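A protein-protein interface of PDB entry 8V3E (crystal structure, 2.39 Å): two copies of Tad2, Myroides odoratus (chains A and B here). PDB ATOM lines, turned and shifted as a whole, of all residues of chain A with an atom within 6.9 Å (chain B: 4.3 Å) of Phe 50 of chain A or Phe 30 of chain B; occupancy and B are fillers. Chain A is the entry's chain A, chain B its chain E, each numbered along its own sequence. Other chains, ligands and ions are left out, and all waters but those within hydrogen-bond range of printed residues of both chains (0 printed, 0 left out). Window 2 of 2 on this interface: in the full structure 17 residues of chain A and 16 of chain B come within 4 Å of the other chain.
Of the 13 printed residues of chain B, 4 touch a printed residue of chain A.
Hydrophobic or aromatic side chains of chain B within 4 Å of the printed part of chain A: Phe 30, Tyr 32 and Ile 69.
Of the 13 printed residues of chain A, 5 touch a printed residue of chain B.
Among the printed residues, no Asp or Glu carboxylate lies within 4 Å of a Lys or Arg side-chain nitrogen of the other chain.
Among the printed residues, merely in contact across the chains: Thr 49 of chain A with Lys 18 of chain B (3.997 Å), Phe 50 of chain A with Phe 30 of chain B (3.96 Å), Phe 50 of chain A with Tyr 32 of chain B (3.9 Å), Phe 50 of chain A with Ile 69 of chain B (3.5 Å), Val 54 of chain A with Ile 69 of chain B (3.5 Å) and Tyr 56 of chain A with Ile 69 of chain B (3.6 Å).
The backbone NH of Ile 69 of chain B sits at hydrogen-bond distance from the backbone carbonyl oxygen of Lys 55 of chain A, 3.1 Å away.
Of chain B, only Phe 30, Tyr 32 and Ile 69 come within 4 Å of Phe 50 of chain A.
Glu 52 of chain A touches none of the printed residues of chain B.
Of the printed residues of chain B, Tyr 56 of chain A touches Ile 69 (3.6 Å).
Of the printed residues of chain A, Lys 18 of chain B touches Thr 49.
Gly 28 of chain B touches none of the printed residues of chain A.
Of chain A, only Phe 50 (3.96 Å) comes within 4 Å of Phe 30 of chain B.
The nearest residue of chain A that does not touch Phe 30 of chain B is Thr 49 of chain A (5.1 Å).
O of Lys 18 of chain B is in hydrogen-bond range of N of Val 87 of chain B, 3.0 Å away.
O of Phe 30 of chain B is in hydrogen-bond range of N of Lys 63 of chain B (2.9 Å).
The backbone NH (N) of Tyr 32 of chain B sits at hydrogen-bond distance from the backbone carbonyl oxygen (O) of Ala 61 of chain B (3.0 Å).
The backbone carbonyl oxygen (O) of Val 45 of chain A sits at hydrogen-bond distance from the side-chain hydroxyl (OG1) of Thr 49 of chain A (3.0 Å).
OG1 of Thr 49 of chain A is in hydrogen-bond range of O of Ile 46 of chain A.
No position is printed for both chains.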
ATOM      1  N   SER A  41     -17.830  -0.763 -21.490  1.00  0.00           N
ATOM      2  CA  SER A  41     -18.722  -1.696 -20.821  1.00  0.00           C
ATOM      3  C   SER A  41     -19.319  -1.054 -19.577  1.00  0.00           C
ATOM      4  O   SER A  41     -18.625  -0.367 -18.819  1.00  0.00           O
ATOM      5  CB  SER A  41     -17.977  -2.976 -20.442  1.00  0.00           C
ATOM      6  OG  SER A  41     -17.362  -3.564 -21.575  1.00  0.00           O
ATOM      7  N   VAL A  45     -21.611  -7.816 -15.656  1.00  0.00           N
ATOM      8  CA  VAL A  45     -21.735  -9.021 -16.471  1.00  0.00           C
ATOM      9  C   VAL A  45     -21.087  -8.814 -17.835  1.00  0.00           C
ATOM     10  O   VAL A  45     -20.518  -9.751 -18.408  1.00  0.00           O
ATOM     11  CB  VAL A  45     -23.215  -9.425 -16.599  1.00  0.00           C
ATOM     12  CG1 VAL A  45     -23.349 -10.735 -17.363  1.00  0.00           C
ATOM     13  CG2 VAL A  45     -23.853  -9.539 -15.225  1.00  0.00           C
ATOM     14  N   ILE A  46     -21.151  -7.595 -18.373  1.00  0.00           N
ATOM     15  CA  ILE A  46     -20.469  -7.312 -19.632  1.00  0.00           C
ATOM     16  C   ILE A  46     -18.962  -7.253 -19.416  1.00  0.00           C
ATOM     17  O   ILE A  46     -18.183  -7.747 -20.239  1.00  0.00           O
ATOM     18  CB  ILE A  46     -21.008  -6.010 -20.254  1.00  0.00           C
ATOM     19  CG1 ILE A  46     -22.533  -6.063 -20.364  1.00  0.00           C
ATOM     20  CG2 ILE A  46     -20.390  -5.778 -21.623  1.00  0.00           C
ATOM     21  CD1 ILE A  46     -23.048  -7.227 -21.179  1.00  0.00           C
ATOM     22  N   LYS A  47     -18.529  -6.656 -18.301  1.00  0.00           N
ATOM     23  CA  LYS A  47     -17.102  -6.593 -18.004  1.00  0.00           C
ATOM     24  C   LYS A  47     -16.527  -7.971 -17.702  1.00  0.00           C
ATOM     25  O   LYS A  47     -15.369  -8.244 -18.033  1.00  0.00           O
ATOM     26  CB  LYS A  47     -16.851  -5.645 -16.830  1.00  0.00           C
ATOM     27  CG  LYS A  47     -17.316  -4.218 -17.070  1.00  0.00           C
ATOM     28  CD  LYS A  47     -17.117  -3.354 -15.835  1.00  0.00           C
ATOM     29  CE  LYS A  47     -17.602  -1.934 -16.069  1.00  0.00           C
ATOM     30  NZ  LYS A  47     -17.459  -1.089 -14.851  1.00  0.00           N
ATOM     31  N   ASN A  48     -17.315  -8.850 -17.081  1.00  0.00           N
ATOM     32  CA  ASN A  48     -16.838 -10.189 -16.759  1.00  0.00           C
ATOM     33  C   ASN A  48     -16.729 -11.092 -17.980  1.00  0.00           C
ATOM     34  O   ASN A  48     -16.129 -12.168 -17.879  1.00  0.00           O
ATOM     35  CB  ASN A  48     -17.751 -10.839 -15.717  1.00  0.00           C
ATOM     36  CG  ASN A  48     -17.452 -10.369 -14.308  1.00  0.00           C
ATOM     37  OD1 ASN A  48     -16.294 -10.151 -13.948  1.00  0.00           O
ATOM     38  ND2 ASN A  48     -18.494 -10.210 -13.502  1.00  0.00           N
ATOM     39  N   THR A  49     -17.284 -10.689 -19.121  1.00  0.00           N
ATOM     40  CA  THR A  49     -17.206 -11.469 -20.349  1.00  0.00           C
ATOM     41  C   THR A  49     -16.391 -10.781 -21.434  1.00  0.00           C
ATOM     42  O   THR A  49     -15.550 -11.420 -22.073  1.00  0.00           O
ATOM     43  CB  THR A  49     -18.617 -11.774 -20.875  1.00  0.00           C
ATOM     44  OG1 THR A  49     -19.347 -10.551 -21.029  1.00  0.00           O
ATOM     45  CG2 THR A  49     -19.360 -12.686 -19.909  1.00  0.00           C
ATOM     46  N   PHE A  50     -16.614  -9.486 -21.657  1.00  0.00           N
ATOM     47  CA  PHE A  50     -15.908  -8.754 -22.700  1.00  0.00           C
ATOM     48  C   PHE A  50     -14.749  -7.916 -22.179  1.00  0.00           C
ATOM     49  O   PHE A  50     -13.842  -7.597 -22.953  1.00  0.00           O
ATOM     50  CB  PHE A  50     -16.879  -7.839 -23.460  1.00  0.00           C
ATOM     51  CG  PHE A  50     -17.939  -8.580 -24.227  1.00  0.00           C
ATOM     52  CD1 PHE A  50     -17.671  -9.086 -25.489  1.00  0.00           C
ATOM     53  CD2 PHE A  50     -19.202  -8.761 -23.692  1.00  0.00           C
ATOM     54  CE1 PHE A  50     -18.642  -9.766 -26.199  1.00  0.00           C
ATOM     55  CE2 PHE A  50     -20.180  -9.440 -24.397  1.00  0.00           C
ATOM     56  CZ  PHE A  50     -19.899  -9.942 -25.653  1.00  0.00           C
ATOM     57  N   GLY A  51     -14.754  -7.552 -20.904  1.00  0.00           N
ATOM     58  CA  GLY A  51     -13.727  -6.695 -20.350  1.00  0.00           C
ATOM     59  C   GLY A  51     -14.235  -5.288 -20.107  1.00  0.00           C
ATOM     60  O   GLY A  51     -15.420  -4.977 -20.258  1.00  0.00           O
ATOM     61  N   GLU A  52     -13.301  -4.417 -19.719  1.00  0.00           N
ATOM     62  CA  GLU A  52     -13.661  -3.029 -19.444  1.00  0.00           C
ATOM     63  C   GLU A  52     -14.106  -2.304 -20.707  1.00  0.00           C
ATOM     64  O   GLU A  52     -15.003  -1.453 -20.658  1.00  0.00           O
ATOM     65  CB  GLU A  52     -12.489  -2.303 -18.789  1.00  0.00           C
ATOM     66  CG  GLU A  52     -12.554  -2.277 -17.272  1.00  0.00           C
ATOM     67  CD  GLU A  52     -13.696  -1.419 -16.756  1.00  0.00           C
ATOM     68  OE1 GLU A  52     -14.088  -0.465 -17.462  1.00  0.00           O
ATOM     69  OE2 GLU A  52     -14.201  -1.696 -15.648  1.00  0.00           O
ATOM     70  N   GLU A  53     -13.494  -2.622 -21.843  1.00  0.00           N
ATOM     71  CA  GLU A  53     -13.887  -2.059 -23.124  1.00  0.00           C
ATOM     72  C   GLU A  53     -14.092  -3.186 -24.125  1.00  0.00           C
ATOM     73  O   GLU A  53     -13.527  -4.274 -23.982  1.00  0.00           O
ATOM     74  CB  GLU A  53     -12.838  -1.066 -23.662  1.00  0.00           C
ATOM     75  CG  GLU A  53     -11.747  -1.701 -24.514  1.00  0.00           C
ATOM     76  CD  GLU A  53     -10.745  -0.688 -25.028  1.00  0.00           C
ATOM     77  OE1 GLU A  53     -10.777   0.469 -24.561  1.00  0.00           O
ATOM     78  OE2 GLU A  53      -9.928  -1.050 -25.899  1.00  0.00           O
ATOM     79  N   VAL A  54     -14.914  -2.919 -25.135  1.00  0.00           N
ATOM     80  CA  VAL A  54     -15.178  -3.867 -26.208  1.00  0.00           C
ATOM     81  C   VAL A  54     -14.954  -3.156 -27.533  1.00  0.00           C
ATOM     82  O   VAL A  54     -15.537  -2.094 -27.782  1.00  0.00           O
ATOM     83  CB  VAL A  54     -16.604  -4.449 -26.118  1.00  0.00           C
ATOM     84  CG1 VAL A  54     -17.636  -3.355 -25.888  1.00  0.00           C
ATOM     85  CG2 VAL A  54     -16.932  -5.236 -27.376  1.00  0.00           C
ATOM     86  N   LYS A  55     -14.089  -3.723 -28.370  1.00  0.00           N
ATOM     87  CA  LYS A  55     -13.780  -3.156 -29.674  1.00  0.00           C
ATOM     88  C   LYS A  55     -14.573  -3.887 -30.748  1.00  0.00           C
ATOM     89  O   LYS A  55     -14.564  -5.122 -30.803  1.00  0.00           O
ATOM     90  CB  LYS A  55     -12.281  -3.234 -29.976  1.00  0.00           C
ATOM     91  CG  LYS A  55     -11.909  -2.666 -31.339  1.00  0.00           C
ATOM     92  CD  LYS A  55     -10.445  -2.251 -31.426  1.00  0.00           C
ATOM     93  CE  LYS A  55      -9.539  -3.403 -31.838  1.00  0.00           C
ATOM     94  NZ  LYS A  55      -9.172  -4.281 -30.694  1.00  0.00           N
ATOM     95  N   TYR A  56     -15.263  -3.124 -31.590  1.00  0.00           N
ATOM     96  CA  TYR A  56     -16.029  -3.666 -32.703  1.00  0.00           C
ATOM     97  C   TYR A  56     -15.257  -3.474 -34.000  1.00  0.00           C
ATOM     98  O   TYR A  56     -14.656  -2.419 -34.229  1.00  0.00           O
ATOM     99  CB  TYR A  56     -17.399  -2.989 -32.810  1.00  0.00           C
ATOM    100  CG  TYR A  56     -18.380  -3.374 -31.724  1.00  0.00           C
ATOM    101  CD1 TYR A  56     -18.209  -2.936 -30.417  1.00  0.00           C
ATOM    102  CD2 TYR A  56     -19.486  -4.164 -32.010  1.00  0.00           C
ATOM    103  CE1 TYR A  56     -19.107  -3.280 -29.424  1.00  0.00           C
ATOM    104  CE2 TYR A  56     -20.389  -4.515 -31.022  1.00  0.00           C
ATOM    105  CZ  TYR A  56     -20.195  -4.070 -29.732  1.00  0.00           C
ATOM    106  OH  TYR A  56     -21.090  -4.415 -28.745  1.00  0.00           O
ATOM    107  N   LYS B  18     -24.696 -17.852 -25.230  1.00  0.00           N
ATOM    108  CA  LYS B  18     -23.533 -17.887 -26.102  1.00  0.00           C
ATOM    109  C   LYS B  18     -23.220 -19.329 -26.473  1.00  0.00           C
ATOM    110  O   LYS B  18     -23.373 -20.239 -25.651  1.00  0.00           O
ATOM    111  CB  LYS B  18     -22.323 -17.241 -25.426  1.00  0.00           C
ATOM    112  CG  LYS B  18     -22.490 -15.755 -25.152  1.00  0.00           C
ATOM    113  CD  LYS B  18     -22.005 -15.403 -23.760  1.00  0.00           C
ATOM    114  CE  LYS B  18     -20.609 -15.943 -23.511  1.00  0.00           C
ATOM    115  NZ  LYS B  18     -20.278 -15.928 -22.059  1.00  0.00           N
ATOM    116  N   VAL B  19     -22.787 -19.538 -27.717  1.00  0.00           N
ATOM    117  CA  VAL B  19     -22.523 -20.872 -28.237  1.00  0.00           C
ATOM    118  C   VAL B  19     -21.158 -20.889 -28.910  1.00  0.00           C
ATOM    119  O   VAL B  19     -20.650 -19.866 -29.370  1.00  0.00           O
ATOM    120  CB  VAL B  19     -23.610 -21.340 -29.228  1.00  0.00           C
ATOM    121  CG1 VAL B  19     -24.956 -21.463 -28.528  1.00  0.00           C
ATOM    122  CG2 VAL B  19     -23.699 -20.383 -30.405  1.00  0.00           C
ATOM    123  N   GLY B  28     -11.628 -19.998 -27.638  1.00  0.00           N
ATOM    124  CA  GLY B  28     -12.175 -18.918 -26.846  1.00  0.00           C
ATOM    125  C   GLY B  28     -13.217 -18.076 -27.541  1.00  0.00           C
ATOM    126  O   GLY B  28     -13.609 -17.035 -27.000  1.00  0.00           O
ATOM    127  N   MET B  29     -13.680 -18.485 -28.717  1.00  0.00           N
ATOM    128  CA  MET B  29     -14.672 -17.724 -29.460  1.00  0.00           C
ATOM    129  C   MET B  29     -16.079 -18.188 -29.107  1.00  0.00           C
ATOM    130  O   MET B  29     -16.301 -19.347 -28.746  1.00  0.00           O
ATOM    131  CB  MET B  29     -14.451 -17.865 -30.967  1.00  0.00           C
ATOM    132  CG  MET B  29     -13.059 -17.486 -31.438  1.00  0.00           C
ATOM    133  SD  MET B  29     -12.912 -17.541 -33.235  1.00  0.00           S
ATOM    134  CE  MET B  29     -13.468 -19.210 -33.568  1.00  0.00           C
ATOM    135  N   PHE B  30     -17.032 -17.266 -29.216  1.00  0.00           N
ATOM    136  CA  PHE B  30     -18.436 -17.610 -29.063  1.00  0.00           C
ATOM    137  C   PHE B  30     -19.271 -16.686 -29.934  1.00  0.00           C
ATOM    138  O   PHE B  30     -18.854 -15.577 -30.278  1.00  0.00           O
ATOM    139  CB  PHE B  30     -18.895 -17.538 -27.597  1.00  0.00           C
ATOM    140  CG  PHE B  30     -18.727 -16.184 -26.960  1.00  0.00           C
ATOM    141  CD1 PHE B  30     -19.660 -15.179 -27.167  1.00  0.00           C
ATOM    142  CD2 PHE B  30     -17.652 -15.926 -26.130  1.00  0.00           C
ATOM    143  CE1 PHE B  30     -19.512 -13.940 -26.577  1.00  0.00           C
ATOM    144  CE2 PHE B  30     -17.501 -14.690 -25.532  1.00  0.00           C
ATOM    145  CZ  PHE B  30     -18.430 -13.696 -25.757  1.00  0.00           C
ATOM    146  N   ALA B  31     -20.459 -17.161 -30.287  1.00  0.00           N
ATOM    147  CA  ALA B  31     -21.429 -16.383 -31.039  1.00  0.00           C
ATOM    148  C   ALA B  31     -22.603 -16.023 -30.138  1.00  0.00           C
ATOM    149  O   ALA B  31     -22.974 -16.788 -29.243  1.00  0.00           O
ATOM    150  CB  ALA B  31     -21.925 -17.150 -32.266  1.00  0.00           C
ATOM    151  N   TYR B  32     -23.182 -14.849 -30.376  1.00  0.00           N
ATOM    152  CA  TYR B  32     -24.326 -14.421 -29.587  1.00  0.00           C
ATOM    153  C   TYR B  32     -25.281 -13.628 -30.467  1.00  0.00           C
ATOM    154  O   TYR B  32     -24.928 -13.167 -31.556  1.00  0.00           O
ATOM    155  CB  TYR B  32     -23.898 -13.605 -28.358  1.00  0.00           C
ATOM    156  CG  TYR B  32     -23.128 -12.341 -28.659  1.00  0.00           C
ATOM    157  CD1 TYR B  32     -21.755 -12.373 -28.868  1.00  0.00           C
ATOM    158  CD2 TYR B  32     -23.771 -11.112 -28.711  1.00  0.00           C
ATOM    159  CE1 TYR B  32     -21.047 -11.215 -29.134  1.00  0.00           C
ATOM    160  CE2 TYR B  32     -23.072  -9.951 -28.976  1.00  0.00           C
ATOM    161  CZ  TYR B  32     -21.711 -10.007 -29.187  1.00  0.00           C
ATOM    162  OH  TYR B  32     -21.012  -8.853 -29.451  1.00  0.00           O
ATOM    163  N   ALA B  61     -23.372 -12.008 -33.813  1.00  0.00           N
ATOM    164  CA  ALA B  61     -22.017 -11.511 -33.639  1.00  0.00           C
ATOM    165  C   ALA B  61     -21.122 -12.629 -33.123  1.00  0.00           C
ATOM    166  O   ALA B  61     -21.592 -13.631 -32.578  1.00  0.00           O
ATOM    167  CB  ALA B  61     -21.977 -10.320 -32.673  1.00  0.00           C
ATOM    168  N   LEU B  62     -19.816 -12.445 -33.301  1.00  0.00           N
ATOM    169  CA  LEU B  62     -18.821 -13.425 -32.884  1.00  0.00           C
ATOM    170  C   LEU B  62     -17.696 -12.704 -32.161  1.00  0.00           C
ATOM    171  O   LEU B  62     -17.079 -11.793 -32.723  1.00  0.00           O
ATOM    172  CB  LEU B  62     -18.270 -14.198 -34.085  1.00  0.00           C
ATOM    173  CG  LEU B  62     -17.281 -15.322 -33.771  1.00  0.00           C
ATOM    174  CD1 LEU B  62     -18.015 -16.630 -33.508  1.00  0.00           C
ATOM    175  CD2 LEU B  62     -16.262 -15.480 -34.893  1.00  0.00           C
ATOM    176  N   LYS B  63     -17.431 -13.106 -30.920  1.00  0.00           N
ATOM    177  CA  LYS B  63     -16.264 -12.615 -30.194  1.00  0.00           C
ATOM    178  C   LYS B  63     -15.054 -13.419 -30.652  1.00  0.00           C
ATOM    179  O   LYS B  63     -14.953 -14.617 -30.368  1.00  0.00           O
ATOM    180  CB  LYS B  63     -16.467 -12.732 -28.686  1.00  0.00           C
ATOM    181  CG  LYS B  63     -15.489 -11.886 -27.878  1.00  0.00           C
ATOM    182  CD  LYS B  63     -14.994 -12.604 -26.632  1.00  0.00           C
ATOM    183  CE  LYS B  63     -13.734 -13.419 -26.905  1.00  0.00           C
ATOM    184  NZ  LYS B  63     -13.951 -14.555 -27.842  1.00  0.00           N
ATOM    185  N   ASN B  67     -10.346 -10.751 -28.939  1.00  0.00           N
ATOM    186  CA  ASN B  67     -11.316 -10.023 -28.119  1.00  0.00           C
ATOM    187  C   ASN B  67     -12.017  -8.940 -28.939  1.00  0.00           C
ATOM    188  O   ASN B  67     -12.337  -7.860 -28.437  1.00  0.00           O
ATOM    189  CB  ASN B  67     -10.666  -9.428 -26.866  1.00  0.00           C
ATOM    190  CG  ASN B  67     -11.019 -10.194 -25.604  1.00  0.00           C
ATOM    191  OD1 ASN B  67     -11.668 -11.238 -25.657  1.00  0.00           O
ATOM    192  ND2 ASN B  67     -10.588  -9.676 -24.459  1.00  0.00           N
ATOM    193  N   ILE B  69     -15.225  -7.959 -31.815  1.00  0.00           N
ATOM    194  CA  ILE B  69     -16.596  -8.288 -32.185  1.00  0.00           C
ATOM    195  C   ILE B  69     -16.726  -8.138 -33.693  1.00  0.00           C
ATOM    196  O   ILE B  69     -16.512  -7.048 -34.238  1.00  0.00           O
ATOM    197  CB  ILE B  69     -17.614  -7.400 -31.454  1.00  0.00           C
ATOM    198  CG1 ILE B  69     -17.496  -7.600 -29.943  1.00  0.00           C
ATOM    199  CG2 ILE B  69     -19.025  -7.711 -31.929  1.00  0.00           C
ATOM    200  CD1 ILE B  69     -17.622  -9.040 -29.506  1.00  0.00           C
ATOM    201  N   VAL B  87     -21.732 -21.917 -23.763  1.00  0.00           N
ATOM    202  CA  VAL B  87     -20.646 -21.408 -22.934  1.00  0.00           C
ATOM    203  C   VAL B  87     -21.228 -20.431 -21.922  1.00  0.00           C
ATOM    204  O   VAL B  87     -22.074 -19.593 -22.263  1.00  0.00           O
ATOM    205  CB  VAL B  87     -19.545 -20.755 -23.798  1.00  0.00           C
ATOM    206  CG1 VAL B  87     -20.004 -20.627 -25.242  1.00  0.00           C
ATOM    207  CG2 VAL B  87     -19.128 -19.396 -23.239  1.00  0.00           C
